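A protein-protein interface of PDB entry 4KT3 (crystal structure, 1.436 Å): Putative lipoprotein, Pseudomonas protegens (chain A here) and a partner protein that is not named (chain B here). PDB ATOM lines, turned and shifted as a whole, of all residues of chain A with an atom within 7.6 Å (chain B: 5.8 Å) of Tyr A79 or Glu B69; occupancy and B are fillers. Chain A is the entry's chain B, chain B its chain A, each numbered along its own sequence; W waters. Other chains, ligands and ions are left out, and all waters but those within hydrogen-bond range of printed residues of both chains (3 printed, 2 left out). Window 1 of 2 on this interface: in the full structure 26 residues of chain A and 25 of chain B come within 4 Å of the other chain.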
ATOM      1  N   PHE A  45     -34.222 -10.527   9.363  1.00  0.00           N
ATOM      2  CA  PHE A  45     -34.584  -9.680   8.228  1.00  0.00           C
ATOM      3  C   PHE A  45     -34.289 -10.356   6.903  1.00  0.00           C
ATOM      4  O   PHE A  45     -33.421 -11.210   6.810  1.00  0.00           O
ATOM      5  CB  PHE A  45     -33.777  -8.388   8.271  1.00  0.00           C
ATOM      6  CG  PHE A  45     -32.297  -8.613   8.190  1.00  0.00           C
ATOM      7  CD1 PHE A  45     -31.686  -8.819   6.967  1.00  0.00           C
ATOM      8  CD2 PHE A  45     -31.524  -8.645   9.338  1.00  0.00           C
ATOM      9  CE1 PHE A  45     -30.335  -9.037   6.876  1.00  0.00           C
ATOM     10  CE2 PHE A  45     -30.165  -8.862   9.262  1.00  0.00           C
ATOM     11  CZ  PHE A  45     -29.563  -9.064   8.030  1.00  0.00           C
ATOM     12  N   ASP A  47     -33.120  -8.895   3.221  1.00  0.00           N
ATOM     13  CA  ASP A  47     -32.593  -7.688   2.600  1.00  0.00           C
ATOM     14  C   ASP A  47     -32.440  -7.897   1.096  1.00  0.00           C
ATOM     15  O   ASP A  47     -31.666  -8.756   0.658  1.00  0.00           O
ATOM     16  CB  ASP A  47     -31.228  -7.387   3.206  1.00  0.00           C
ATOM     17  CG  ASP A  47     -30.686  -6.031   2.820  1.00  0.00           C
ATOM     18  OD1 ASP A  47     -31.250  -5.361   1.938  1.00  0.00           O
ATOM     19  OD2 ASP A  47     -29.661  -5.641   3.413  1.00  0.00           O
ATOM     20  N   LEU A  50     -29.197  -5.619  -2.628  1.00  0.00           N
ATOM     21  CA  LEU A  50     -27.935  -6.207  -3.032  1.00  0.00           C
ATOM     22  C   LEU A  50     -27.667  -5.763  -4.468  1.00  0.00           C
ATOM     23  O   LEU A  50     -28.493  -5.987  -5.358  1.00  0.00           O
ATOM     24  CB  LEU A  50     -28.013  -7.725  -2.944  1.00  0.00           C
ATOM     25  CG  LEU A  50     -28.339  -8.314  -1.574  1.00  0.00           C
ATOM     26  CD1 LEU A  50     -28.195  -9.834  -1.613  1.00  0.00           C
ATOM     27  CD2 LEU A  50     -27.473  -7.729  -0.490  1.00  0.00           C
ATOM     28  N   SER A  66     -30.653 -11.430   0.929  1.00  0.00           N
ATOM     29  CA  SER A  66     -29.986 -12.064   2.055  1.00  0.00           C
ATOM     30  C   SER A  66     -30.974 -12.248   3.195  1.00  0.00           C
ATOM     31  O   SER A  66     -31.891 -11.444   3.375  1.00  0.00           O
ATOM     32  CB  SER A  66     -28.795 -11.231   2.520  1.00  0.00           C
ATOM     33  OG  SER A  66     -29.218 -10.032   3.119  1.00  0.00           O
ATOM     34  N   LEU A  67     -30.785 -13.326   3.952  1.00  0.00           N
ATOM     35  CA  LEU A  67     -31.570 -13.611   5.137  1.00  0.00           C
ATOM     36  C   LEU A  67     -30.614 -13.576   6.317  1.00  0.00           C
ATOM     37  O   LEU A  67     -29.606 -14.285   6.341  1.00  0.00           O
ATOM     38  CB  LEU A  67     -32.205 -14.983   5.022  1.00  0.00           C
ATOM     39  CG  LEU A  67     -32.952 -15.490   6.256  1.00  0.00           C
ATOM     40  CD1 LEU A  67     -34.143 -14.601   6.588  1.00  0.00           C
ATOM     41  CD2 LEU A  67     -33.385 -16.927   6.026  1.00  0.00           C
ATOM     42  N   GLY A  68     -30.910 -12.733   7.290  1.00  0.00           N
ATOM     43  CA  GLY A  68     -29.976 -12.518   8.373  1.00  0.00           C
ATOM     44  C   GLY A  68     -30.623 -12.251   9.707  1.00  0.00           C
ATOM     45  O   GLY A  68     -31.841 -12.152   9.814  1.00  0.00           O
ATOM     46  N   TYR A  69     -29.769 -12.087  10.711  1.00  0.00           N
ATOM     47  CA  TYR A  69     -30.182 -12.058  12.087  1.00  0.00           C
ATOM     48  C   TYR A  69     -29.194 -11.247  12.913  1.00  0.00           C
ATOM     49  O   TYR A  69     -28.001 -11.542  12.906  1.00  0.00           O
ATOM     50  CB  TYR A  69     -30.220 -13.501  12.588  1.00  0.00           C
ATOM     51  CG  TYR A  69     -30.488 -13.644  14.058  1.00  0.00           C
ATOM     52  CD1 TYR A  69     -31.607 -13.067  14.622  1.00  0.00           C
ATOM     53  CD2 TYR A  69     -29.631 -14.376  14.877  1.00  0.00           C
ATOM     54  CE1 TYR A  69     -31.881 -13.194  15.957  1.00  0.00           C
ATOM     55  CE2 TYR A  69     -29.893 -14.513  16.228  1.00  0.00           C
ATOM     56  CZ  TYR A  69     -31.027 -13.912  16.765  1.00  0.00           C
ATOM     57  OH  TYR A  69     -31.341 -14.020  18.107  1.00  0.00           O
ATOM     58  N   ASN A  70     -29.691 -10.244  13.642  1.00  0.00           N
ATOM     59  CA  ASN A  70     -28.852  -9.503  14.591  1.00  0.00           C
ATOM     60  C   ASN A  70     -29.266  -9.811  16.026  1.00  0.00           C
ATOM     61  O   ASN A  70     -30.414  -9.566  16.438  1.00  0.00           O
ATOM     62  CB  ASN A  70     -28.907  -7.990  14.346  1.00  0.00           C
ATOM     63  CG  ASN A  70     -28.128  -7.559  13.119  1.00  0.00           C
ATOM     64  OD1 ASN A  70     -26.902  -7.709  13.056  1.00  0.00           O
ATOM     65  ND2 ASN A  70     -28.836  -7.013  12.133  1.00  0.00           N
ATOM     66  N   GLY A  75     -21.511 -10.158  18.122  1.00  0.00           N
ATOM     67  CA  GLY A  75     -20.709  -9.003  17.781  1.00  0.00           C
ATOM     68  C   GLY A  75     -20.820  -8.613  16.319  1.00  0.00           C
ATOM     69  O   GLY A  75     -20.221  -7.618  15.911  1.00  0.00           O
ATOM     70  N   ALA A  76     -21.616  -9.365  15.555  1.00  0.00           N
ATOM     71  CA  ALA A  76     -21.764  -9.133  14.117  1.00  0.00           C
ATOM     72  C   ALA A  76     -23.054  -9.772  13.638  1.00  0.00           C
ATOM     73  O   ALA A  76     -23.626 -10.627  14.314  1.00  0.00           O
ATOM     74  CB  ALA A  76     -20.574  -9.735  13.358  1.00  0.00           C
ATOM     75  N   THR A  77     -23.523  -9.349  12.471  1.00  0.00           N
ATOM     76  CA  THR A  77     -24.704  -9.953  11.887  1.00  0.00           C
ATOM     77  C   THR A  77     -24.422 -11.408  11.540  1.00  0.00           C
ATOM     78  O   THR A  77     -23.321 -11.764  11.122  1.00  0.00           O
ATOM     79  CB  THR A  77     -25.169  -9.179  10.641  1.00  0.00           C
ATOM     80  OG1 THR A  77     -25.230  -7.780  10.944  1.00  0.00           O
ATOM     81  CG2 THR A  77     -26.527  -9.667  10.150  1.00  0.00           C
ATOM     82  N   GLU A  78     -25.434 -12.245  11.708  1.00  0.00           N
ATOM     83  CA  GLU A  78     -25.346 -13.644  11.336  1.00  0.00           C
ATOM     84  C   GLU A  78     -26.221 -13.861  10.111  1.00  0.00           C
ATOM     85  O   GLU A  78     -27.395 -13.483  10.116  1.00  0.00           O
ATOM     86  CB  GLU A  78     -25.825 -14.524  12.495  1.00  0.00           C
ATOM     87  CG  GLU A  78     -25.845 -16.008  12.209  1.00  0.00           C
ATOM     88  CD  GLU A  78     -26.206 -16.834  13.445  1.00  0.00           C
ATOM     89  OE1 GLU A  78     -25.748 -16.492  14.553  1.00  0.00           O
ATOM     90  OE2 GLU A  78     -26.975 -17.814  13.325  1.00  0.00           O
ATOM     91  N   TYR A  79     -25.676 -14.490   9.078  1.00  0.00           N
ATOM     92  CA  TYR A  79     -26.438 -14.695   7.840  1.00  0.00           C
ATOM     93  C   TYR A  79     -26.796 -16.164   7.633  1.00  0.00           C
ATOM     94  O   TYR A  79     -25.996 -17.061   7.887  1.00  0.00           O
ATOM     95  CB  TYR A  79     -25.677 -14.125   6.646  1.00  0.00           C
ATOM     96  CG  TYR A  79     -25.498 -12.629   6.763  1.00  0.00           C
ATOM     97  CD1 TYR A  79     -26.478 -11.756   6.312  1.00  0.00           C
ATOM     98  CD2 TYR A  79     -24.371 -12.091   7.381  1.00  0.00           C
ATOM     99  CE1 TYR A  79     -26.321 -10.381   6.442  1.00  0.00           C
ATOM    100  CE2 TYR A  79     -24.205 -10.738   7.506  1.00  0.00           C
ATOM    101  CZ  TYR A  79     -25.183  -9.884   7.046  1.00  0.00           C
ATOM    102  OH  TYR A  79     -25.004  -8.541   7.171  1.00  0.00           O
ATOM    103  N   TRP A  80     -28.031 -16.394   7.215  1.00  0.00           N
ATOM    104  CA  TRP A  80     -28.572 -17.737   7.099  1.00  0.00           C
ATOM    105  C   TRP A  80     -28.748 -18.161   5.643  1.00  0.00           C
ATOM    106  O   TRP A  80     -28.882 -19.347   5.347  1.00  0.00           O
ATOM    107  CB  TRP A  80     -29.930 -17.799   7.805  1.00  0.00           C
ATOM    108  CG  TRP A  80     -29.855 -17.648   9.304  1.00  0.00           C
ATOM    109  CD1 TRP A  80     -28.756 -17.804  10.098  1.00  0.00           C
ATOM    110  CD2 TRP A  80     -30.940 -17.322  10.176  1.00  0.00           C
ATOM    111  NE1 TRP A  80     -29.096 -17.593  11.420  1.00  0.00           N
ATOM    112  CE2 TRP A  80     -30.430 -17.290  11.491  1.00  0.00           C
ATOM    113  CE3 TRP A  80     -32.292 -17.044   9.972  1.00  0.00           C
ATOM    114  CZ2 TRP A  80     -31.227 -16.999  12.599  1.00  0.00           C
ATOM    115  CZ3 TRP A  80     -33.085 -16.756  11.074  1.00  0.00           C
ATOM    116  CH2 TRP A  80     -32.549 -16.734  12.369  1.00  0.00           C
ATOM    117  N   GLY A  81     -28.781 -17.197   4.735  1.00  0.00           N
ATOM    118  CA  GLY A  81     -28.924 -17.525   3.331  1.00  0.00           C
ATOM    119  C   GLY A  81     -28.692 -16.356   2.392  1.00  0.00           C
ATOM    120  O   GLY A  81     -28.911 -15.198   2.749  1.00  0.00           O
ATOM    121  N   LEU A  82     -28.264 -16.687   1.178  1.00  0.00           N
ATOM    122  CA  LEU A  82     -28.170 -15.750   0.072  1.00  0.00           C
ATOM    123  C   LEU A  82     -28.933 -16.408  -1.064  1.00  0.00           C
ATOM    124  O   LEU A  82     -28.584 -17.504  -1.491  1.00  0.00           O
ATOM    125  CB  LEU A  82     -26.711 -15.507  -0.337  1.00  0.00           C
ATOM    126  CG  LEU A  82     -26.499 -14.626  -1.580  1.00  0.00           C
ATOM    127  CD1 LEU A  82     -27.129 -13.249  -1.420  1.00  0.00           C
ATOM    128  CD2 LEU A  82     -25.001 -14.470  -1.904  1.00  0.00           C
ATOM    129  N   GLU A  94     -30.667 -21.022  -3.307  1.00  0.00           N
ATOM    130  CA  GLU A  94     -29.709 -20.573  -2.306  1.00  0.00           C
ATOM    131  C   GLU A  94     -28.345 -20.773  -2.961  1.00  0.00           C
ATOM    132  O   GLU A  94     -27.971 -21.904  -3.280  1.00  0.00           O
ATOM    133  CB  GLU A  94     -29.831 -21.397  -1.028  1.00  0.00           C
ATOM    134  CG  GLU A  94     -29.454 -20.635   0.240  1.00  0.00           C
ATOM    135  CD  GLU A  94     -27.960 -20.402   0.374  1.00  0.00           C
ATOM    136  OE1 GLU A  94     -27.184 -21.156  -0.237  1.00  0.00           O
ATOM    137  OE2 GLU A  94     -27.554 -19.455   1.085  1.00  0.00           O
ATOM    138  N   ASN A  96     -25.101 -20.124  -2.117  1.00  0.00           N
ATOM    139  CA  ASN A  96     -23.898 -20.587  -1.438  1.00  0.00           C
ATOM    140  C   ASN A  96     -23.901 -22.113  -1.296  1.00  0.00           C
ATOM    141  O   ASN A  96     -22.926 -22.772  -1.643  1.00  0.00           O
ATOM    142  CB  ASN A  96     -23.752 -19.895  -0.084  1.00  0.00           C
ATOM    143  CG  ASN A  96     -23.231 -18.493  -0.223  1.00  0.00           C
ATOM    144  OD1 ASN A  96     -22.426 -18.214  -1.115  1.00  0.00           O
ATOM    145  ND2 ASN A  96     -23.683 -17.599   0.639  1.00  0.00           N
ATOM    146  N   GLY B  64     -13.540 -15.886   3.087  1.00  0.00           N
ATOM    147  CA  GLY B  64     -14.814 -16.598   3.123  1.00  0.00           C
ATOM    148  C   GLY B  64     -15.780 -15.974   4.114  1.00  0.00           C
ATOM    149  O   GLY B  64     -16.975 -15.839   3.831  1.00  0.00           O
ATOM    150  N   LEU B  65     -15.280 -15.610   5.292  1.00  0.00           N
ATOM    151  CA  LEU B  65     -16.113 -14.918   6.266  1.00  0.00           C
ATOM    152  C   LEU B  65     -16.614 -13.594   5.685  1.00  0.00           C
ATOM    153  O   LEU B  65     -17.809 -13.286   5.798  1.00  0.00           O
ATOM    154  CB  LEU B  65     -15.401 -14.715   7.602  1.00  0.00           C
ATOM    155  CG  LEU B  65     -16.230 -13.980   8.666  1.00  0.00           C
ATOM    156  CD1 LEU B  65     -17.535 -14.701   8.987  1.00  0.00           C
ATOM    157  CD2 LEU B  65     -15.393 -13.789   9.932  1.00  0.00           C
ATOM    158  N   ALA B  66     -15.740 -12.830   5.035  1.00  0.00           N
ATOM    159  CA  ALA B  66     -16.185 -11.582   4.418  1.00  0.00           C
ATOM    160  C   ALA B  66     -17.253 -11.850   3.340  1.00  0.00           C
ATOM    161  O   ALA B  66     -18.207 -11.089   3.208  1.00  0.00           O
ATOM    162  CB  ALA B  66     -15.014 -10.829   3.837  1.00  0.00           C
ATOM    163  N   ALA B  67     -17.079 -12.907   2.550  1.00  0.00           N
ATOM    164  CA  ALA B  67     -18.060 -13.245   1.508  1.00  0.00           C
ATOM    165  C   ALA B  67     -19.436 -13.548   2.114  1.00  0.00           C
ATOM    166  O   ALA B  67     -20.466 -13.177   1.553  1.00  0.00           O
ATOM    167  CB  ALA B  67     -17.579 -14.428   0.686  1.00  0.00           C
ATOM    168  N   GLN B  68     -19.440 -14.274   3.224  1.00  0.00           N
ATOM    169  CA  GLN B  68     -20.652 -14.579   3.977  1.00  0.00           C
ATOM    170  C   GLN B  68     -21.327 -13.314   4.519  1.00  0.00           C
ATOM    171  O   GLN B  68     -22.537 -13.141   4.406  1.00  0.00           O
ATOM    172  CB  GLN B  68     -20.266 -15.506   5.139  1.00  0.00           C
ATOM    173  CG  GLN B  68     -21.220 -15.555   6.331  1.00  0.00           C
ATOM    174  CD  GLN B  68     -22.528 -16.273   6.042  1.00  0.00           C
ATOM    175  OE1 GLN B  68     -22.964 -16.381   4.894  1.00  0.00           O
ATOM    176  NE2 GLN B  68     -23.178 -16.753   7.104  1.00  0.00           N
ATOM    177  N   GLU B  69     -20.552 -12.429   5.134  1.00  0.00           N
ATOM    178  CA  GLU B  69     -21.140 -11.269   5.792  1.00  0.00           C
ATOM    179  C   GLU B  69     -21.618 -10.218   4.806  1.00  0.00           C
ATOM    180  O   GLU B  69     -22.602  -9.512   5.073  1.00  0.00           O
ATOM    181  CB  GLU B  69     -20.136 -10.625   6.749  1.00  0.00           C
ATOM    182  CG  GLU B  69     -19.658 -11.533   7.888  1.00  0.00           C
ATOM    183  CD  GLU B  69     -20.788 -11.955   8.786  1.00  0.00           C
ATOM    184  OE1 GLU B  69     -21.411 -11.067   9.420  1.00  0.00           O
ATOM    185  OE2 GLU B  69     -21.038 -13.170   8.852  1.00  0.00           O
ATOM    186  N   SER B  70     -20.907 -10.098   3.686  1.00  0.00           N
ATOM    187  CA  SER B  70     -21.145  -9.029   2.713  1.00  0.00           C
ATOM    188  C   SER B  70     -21.871  -9.448   1.442  1.00  0.00           C
ATOM    189  O   SER B  70     -22.031  -8.630   0.546  1.00  0.00           O
ATOM    190  CB  SER B  70     -19.807  -8.378   2.329  1.00  0.00           C
ATOM    191  OG  SER B  70     -19.039  -9.205   1.472  1.00  0.00           O
ATOM    192  N   GLN B  71     -22.270 -10.715   1.368  1.00  0.00           N
ATOM    193  CA  GLN B  71     -22.895 -11.262   0.164  1.00  0.00           C
ATOM    194  C   GLN B  71     -21.976 -10.991  -1.041  1.00  0.00           C
ATOM    195  O   GLN B  71     -22.371 -10.435  -2.077  1.00  0.00           O
ATOM    196  CB  GLN B  71     -24.300 -10.676  -0.047  1.00  0.00           C
ATOM    197  CG  GLN B  71     -25.300 -11.051   1.069  1.00  0.00           C
ATOM    198  CD  GLN B  71     -25.014 -10.349   2.397  1.00  0.00           C
ATOM    199  OE1 GLN B  71     -24.854 -10.994   3.457  1.00  0.00           O
ATOM    200  NE2 GLN B  71     -24.945  -9.039   2.351  1.00  0.00           N
ATOM    201  N   ILE B  77     -24.220  -2.665   3.727  1.00  0.00           N
ATOM    202  CA  ILE B  77     -23.290  -2.352   4.806  1.00  0.00           C
ATOM    203  C   ILE B  77     -21.845  -2.393   4.292  1.00  0.00           C
ATOM    204  O   ILE B  77     -20.996  -1.593   4.689  1.00  0.00           O
ATOM    205  CB  ILE B  77     -23.536  -3.311   6.015  1.00  0.00           C
ATOM    206  CG1 ILE B  77     -24.863  -2.926   6.691  1.00  0.00           C
ATOM    207  CG2 ILE B  77     -22.383  -3.287   6.992  1.00  0.00           C
ATOM    208  CD1 ILE B  77     -25.436  -4.022   7.576  1.00  0.00           C
ATOM    209  N   ASN B  83     -18.061  -2.060   5.681  1.00  0.00           N
ATOM    210  CA  ASN B  83     -18.045  -2.991   6.802  1.00  0.00           C
ATOM    211  C   ASN B  83     -18.291  -4.387   6.260  1.00  0.00           C
ATOM    212  O   ASN B  83     -19.439  -4.846   6.205  1.00  0.00           O
ATOM    213  CB  ASN B  83     -19.089  -2.576   7.836  1.00  0.00           C
ATOM    214  CG  ASN B  83     -19.096  -3.457   9.078  1.00  0.00           C
ATOM    215  OD1 ASN B  83     -18.432  -4.495   9.152  1.00  0.00           O
ATOM    216  ND2 ASN B  83     -19.890  -3.048  10.068  1.00  0.00           N
ATOM    217  N   TYR B  84     -17.206  -5.044   5.853  1.00  0.00           N
ATOM    218  CA  TYR B  84     -17.300  -6.335   5.161  1.00  0.00           C
ATOM    219  C   TYR B  84     -17.417  -7.520   6.120  1.00  0.00           C
ATOM    220  O   TYR B  84     -17.503  -8.659   5.680  1.00  0.00           O
ATOM    221  CB  TYR B  84     -16.141  -6.514   4.178  1.00  0.00           C
ATOM    222  CG  TYR B  84     -16.257  -5.661   2.948  1.00  0.00           C
ATOM    223  CD1 TYR B  84     -15.900  -4.320   2.973  1.00  0.00           C
ATOM    224  CD2 TYR B  84     -16.709  -6.193   1.749  1.00  0.00           C
ATOM    225  CE1 TYR B  84     -16.009  -3.528   1.837  1.00  0.00           C
ATOM    226  CE2 TYR B  84     -16.819  -5.414   0.623  1.00  0.00           C
ATOM    227  CZ  TYR B  84     -16.473  -4.081   0.674  1.00  0.00           C
ATOM    228  OH  TYR B  84     -16.592  -3.297  -0.461  1.00  0.00           O
ATOM    229  N   PHE B  85     -17.461  -7.249   7.423  1.00  0.00           N
ATOM    230  CA  PHE B  85     -17.624  -8.306   8.423  1.00  0.00           C
ATOM    231  C   PHE B  85     -18.880  -8.085   9.254  1.00  0.00           C
ATOM    232  O   PHE B  85     -19.095  -8.758  10.270  1.00  0.00           O
ATOM    233  CB  PHE B  85     -16.345  -8.402   9.276  1.00  0.00           C
ATOM    234  CG  PHE B  85     -15.178  -8.919   8.486  1.00  0.00           C
ATOM    235  CD1 PHE B  85     -14.439  -8.062   7.683  1.00  0.00           C
ATOM    236  CD2 PHE B  85     -14.867 -10.272   8.476  1.00  0.00           C
ATOM    237  CE1 PHE B  85     -13.420  -8.535   6.900  1.00  0.00           C
ATOM    238  CE2 PHE B  85     -13.822 -10.747   7.698  1.00  0.00           C
ATOM    239  CZ  PHE B  85     -13.103  -9.873   6.909  1.00  0.00           C
ATOM    240  N   SER B  86     -19.719  -7.157   8.777  1.00  0.00           N
ATOM    241  CA  SER B  86     -20.957  -6.758   9.448  1.00  0.00           C
ATOM    242  C   SER B  86     -20.795  -6.642  10.964  1.00  0.00           C
ATOM    243  O   SER B  86     -21.629  -7.128  11.737  1.00  0.00           O
ATOM    244  CB  SER B  86     -22.107  -7.710   9.092  1.00  0.00           C
ATOM    245  OG  SER B  86     -22.336  -7.695   7.695  1.00  0.00           O
ATOM    246  N   MET B  87     -19.725  -5.968  11.370  1.00  0.00           N
ATOM    247  CA  MET B  87     -19.422  -5.745  12.773  1.00  0.00           C
ATOM    248  C   MET B  87     -20.432  -4.813  13.394  1.00  0.00           C
ATOM    249  O   MET B  87     -20.686  -3.733  12.872  1.00  0.00           O
ATOM    250  CB  MET B  87     -18.052  -5.077  12.913  1.00  0.00           C
ATOM    251  CG  MET B  87     -16.920  -5.837  12.270  1.00  0.00           C
ATOM    252  SD  MET B  87     -16.306  -7.326  13.349  1.00  0.00           S
ATOM    253  CE  MET B  87     -15.438  -6.337  14.775  1.00  0.00           C
ATOM    254  N   TYR B 147     -18.800 -13.965  18.136  1.00  0.00           N
ATOM    255  CA  TYR B 147     -18.973 -13.243  16.884  1.00  0.00           C
ATOM    256  C   TYR B 147     -20.403 -13.423  16.359  1.00  0.00           C
ATOM    257  O   TYR B 147     -21.084 -12.449  16.007  1.00  0.00           O
ATOM    258  CB  TYR B 147     -17.958 -13.748  15.849  1.00  0.00           C
ATOM    259  CG  TYR B 147     -18.107 -13.119  14.477  1.00  0.00           C
ATOM    260  CD1 TYR B 147     -18.837 -13.741  13.476  1.00  0.00           C
ATOM    261  CD2 TYR B 147     -17.521 -11.902  14.192  1.00  0.00           C
ATOM    262  CE1 TYR B 147     -18.959 -13.159  12.208  1.00  0.00           C
ATOM    263  CE2 TYR B 147     -17.647 -11.310  12.945  1.00  0.00           C
ATOM    264  CZ  TYR B 147     -18.352 -11.947  11.957  1.00  0.00           C
ATOM    265  OH  TYR B 147     -18.488 -11.372  10.716  1.00  0.00           O
ATOM    266  N   ASN B 148     -20.832 -14.676  16.281  1.00  0.00           N
ATOM    267  CA  ASN B 148     -22.227 -15.019  16.018  1.00  0.00           C
ATOM    268  C   ASN B 148     -22.609 -16.025  17.082  1.00  0.00           C
ATOM    269  O   ASN B 148     -21.756 -16.783  17.542  1.00  0.00           O
ATOM    270  CB  ASN B 148     -22.412 -15.700  14.652  1.00  0.00           C
ATOM    271  CG  ASN B 148     -22.353 -14.750  13.472  1.00  0.00           C
ATOM    272  OD1 ASN B 148     -22.361 -13.523  13.587  1.00  0.00           O
ATOM    273  ND2 ASN B 148     -22.331 -15.341  12.326  1.00  0.00           N
ATOM    274  N   PHE B 160     -24.676 -23.938  11.122  1.00  0.00           N
ATOM    275  CA  PHE B 160     -23.883 -22.740  10.889  1.00  0.00           C
ATOM    276  C   PHE B 160     -22.480 -23.080  10.384  1.00  0.00           C
ATOM    277  O   PHE B 160     -22.001 -22.500   9.400  1.00  0.00           O
ATOM    278  CB  PHE B 160     -23.781 -21.904  12.169  1.00  0.00           C
ATOM    279  CG  PHE B 160     -22.843 -20.746  12.051  1.00  0.00           C
ATOM    280  CD1 PHE B 160     -21.526 -20.849  12.495  1.00  0.00           C
ATOM    281  CD2 PHE B 160     -23.264 -19.558  11.479  1.00  0.00           C
ATOM    282  CE1 PHE B 160     -20.654 -19.784  12.373  1.00  0.00           C
ATOM    283  CE2 PHE B 160     -22.397 -18.494  11.352  1.00  0.00           C
ATOM    284  CZ  PHE B 160     -21.088 -18.605  11.803  1.00  0.00           C
ATOM    285  N   TYR B 163     -22.218 -24.633   6.811  1.00  0.00           N
ATOM    286  CA  TYR B 163     -22.592 -23.630   5.825  1.00  0.00           C
ATOM    287  C   TYR B 163     -21.420 -22.666   5.570  1.00  0.00           C
ATOM    288  O   TYR B 163     -21.066 -22.398   4.421  1.00  0.00           O
ATOM    289  CB  TYR B 163     -23.859 -22.883   6.278  1.00  0.00           C
ATOM    290  CG  TYR B 163     -24.333 -21.815   5.307  1.00  0.00           C
ATOM    291  CD1 TYR B 163     -23.911 -20.499   5.431  1.00  0.00           C
ATOM    292  CD2 TYR B 163     -25.196 -22.124   4.271  1.00  0.00           C
ATOM    293  CE1 TYR B 163     -24.328 -19.519   4.532  1.00  0.00           C
ATOM    294  CE2 TYR B 163     -25.628 -21.156   3.376  1.00  0.00           C
ATOM    295  CZ  TYR B 163     -25.193 -19.857   3.515  1.00  0.00           C
ATOM    296  OH  TYR B 163     -25.610 -18.887   2.640  1.00  0.00           O
HETATM  297  O   HOH W   1     -25.580 -16.362   3.993  1.00  0.00           O
HETATM  298  O   HOH W   2     -22.808 -14.810   0.888  1.00  0.00           O
HETATM  299  O   HOH W   3     -27.574  -8.083   3.617  1.00  0.00           O
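The side-chain amide nitrogen (ND2) of Asn A96 lies within hydrogen-bond range of the side-chain hydroxyl (OH) of Tyr B163, at 3.1 Å.
The backbone carbonyl oxygen (O) of Ala A76 sits close to the side-chain amide oxygen (OD1) of Asn B148, at 3.2 Å.
O of Tyr B147 lies within hydrogen-bond range of N of Ala A76 (3.2 Å).
The backbone carbonyl oxygen (O) of Ser B86 lies within hydrogen-bond range of the backbone NH (N) of Thr A77 (3.0 Å).
The backbone carbonyl oxygen (O) of Tyr B147 is in hydrogen-bond range of the backbone NH (N) of Gly A75 (3.1 Å).
The side-chain hydroxyl (OH) of Tyr A79 lies close to the backbone carbonyl oxygen (O) of Glu B69, at 3.3 Å.
OE2 of Glu A94 is in hydrogen-bond range of OH of Tyr B163 (2.6 Å).
O of Thr A77 lies close to OE1 of Glu B69 (2.7 Å).
The backbone carbonyl oxygen of Thr A77 sits close to the side-chain amide oxygen of Asn B148 (3.2 Å).
The side-chain amide nitrogen (NE2) of Gln B68 lies within hydrogen-bond range of the backbone carbonyl oxygen (O) of Tyr A79 (2.9 Å).
The side-chain hydroxyl of Ser B86 lies within hydrogen-bond range of the side-chain hydroxyl of Tyr A79 (2.8 Å).
CB of Ser A66 touches CG of Gln B71, at 3.8 Å.
Gly A75 touches Met B87 (O to CA, 3.7 Å).
O of Phe B85 touches CB of Ala A76 (3.6 Å).
Ala A76 touches Ser B86.
CB of Asn B148 touches OE1 of Glu A78 (3.4 Å).
Gln B71 touches Tyr A79.
OH of Tyr B163 touches CA of Gly A81, at 3.6 Å.
CD1 of Leu A82 touches CG of Gln B71, at 3.8 Å.
Leu A82 touches Tyr B163 (N to OH, 3.7 Å).
Water W3 lies within hydrogen-bond range of the side-chain hydroxyl of Ser A66 (2.6 Å), the side-chain amide nitrogen of Gln B71 (3.1 Å) and the side-chain carboxylate of Asp A47 (3.2 Å).
Water W1 lies within hydrogen-bond range of OE1 of Gln B68, OH of Tyr B163 and N of Gly A81.
Water W2 lies within hydrogen-bond range of O of Ala B67 (2.9 Å) and ND2 of Asn A96 (2.9 Å).
Printed residues of chain A that touch a printed residue of chain B: Ser A66, Gly A75, Ala A76, Thr A77, Glu A78, Tyr A79, Gly A81, Leu A82, Glu A94 and Asn A96.
Hydrophobic or aromatic side chains of chain A that line the printed part of chain B: Ala A76, Tyr A79 and Leu A82.
Printed residues of chain B that touch a printed residue of chain A: Gln B68, Glu B69, Gln B71, Phe B85, Ser B86, Met B87, Tyr B147, Asn B148 and Tyr B163.
Hydrophobic or aromatic side chains of chain B that line the printed part of chain A: Tyr B147 and Tyr B163.
Among the printed residues, 20 pairs touch across the chains.
Among the printed residues, no Asp or Glu carboxylate lies within 4 Å of a Lys or Arg side-chain nitrogen of the other chain.
The side-chain amide oxygen (OD1) of Asn A70 sits at hydrogen-bond distance from the side-chain hydroxyl (OG1) of Thr A77 (2.7 Å).
The backbone NH (N) of Leu A82 sits at hydrogen-bond distance from the side-chain carboxylate (OE2) of Glu A94 (2.9 Å).
The backbone carbonyl oxygen (O) of Gln B68 lies close to the side-chain amide oxygen (OE1) of Gln B71 (3.3 Å).
OD1 of Asn B83 is in hydrogen-bond range of N of Met B87, at 3.0 Å.
O of Ser A66 sits at hydrogen-bond distance from N of Asp A47 (2.8 Å).
The backbone carbonyl oxygen (O) of Gly A81 sits at hydrogen-bond distance from the backbone NH (N) of Leu A67 (2.9 Å).
Tyr A79 touches just these residues of chain B: Gln B68, Glu B69, Gln B71 and Ser B86.
Of chain A, only Thr A77 and Tyr A79 come within 4 Å of Glu B69.
Printed residues of chain A within 4 Å of Ser B86: Ala A76, Thr A77 and Tyr A79.
Of the printed residues of chain B, Asn A96 touches Tyr B163.
Of the printed residues of chain A, Tyr B163 touches Gly A81 (3.6 Å), Leu A82 (3.7 Å), Glu A94 (2.6 Å) and Asn A96 (3.1 Å).
The nearest residue of chain A that does not touch Glu B69 is Ala A76 (4.2 Å).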
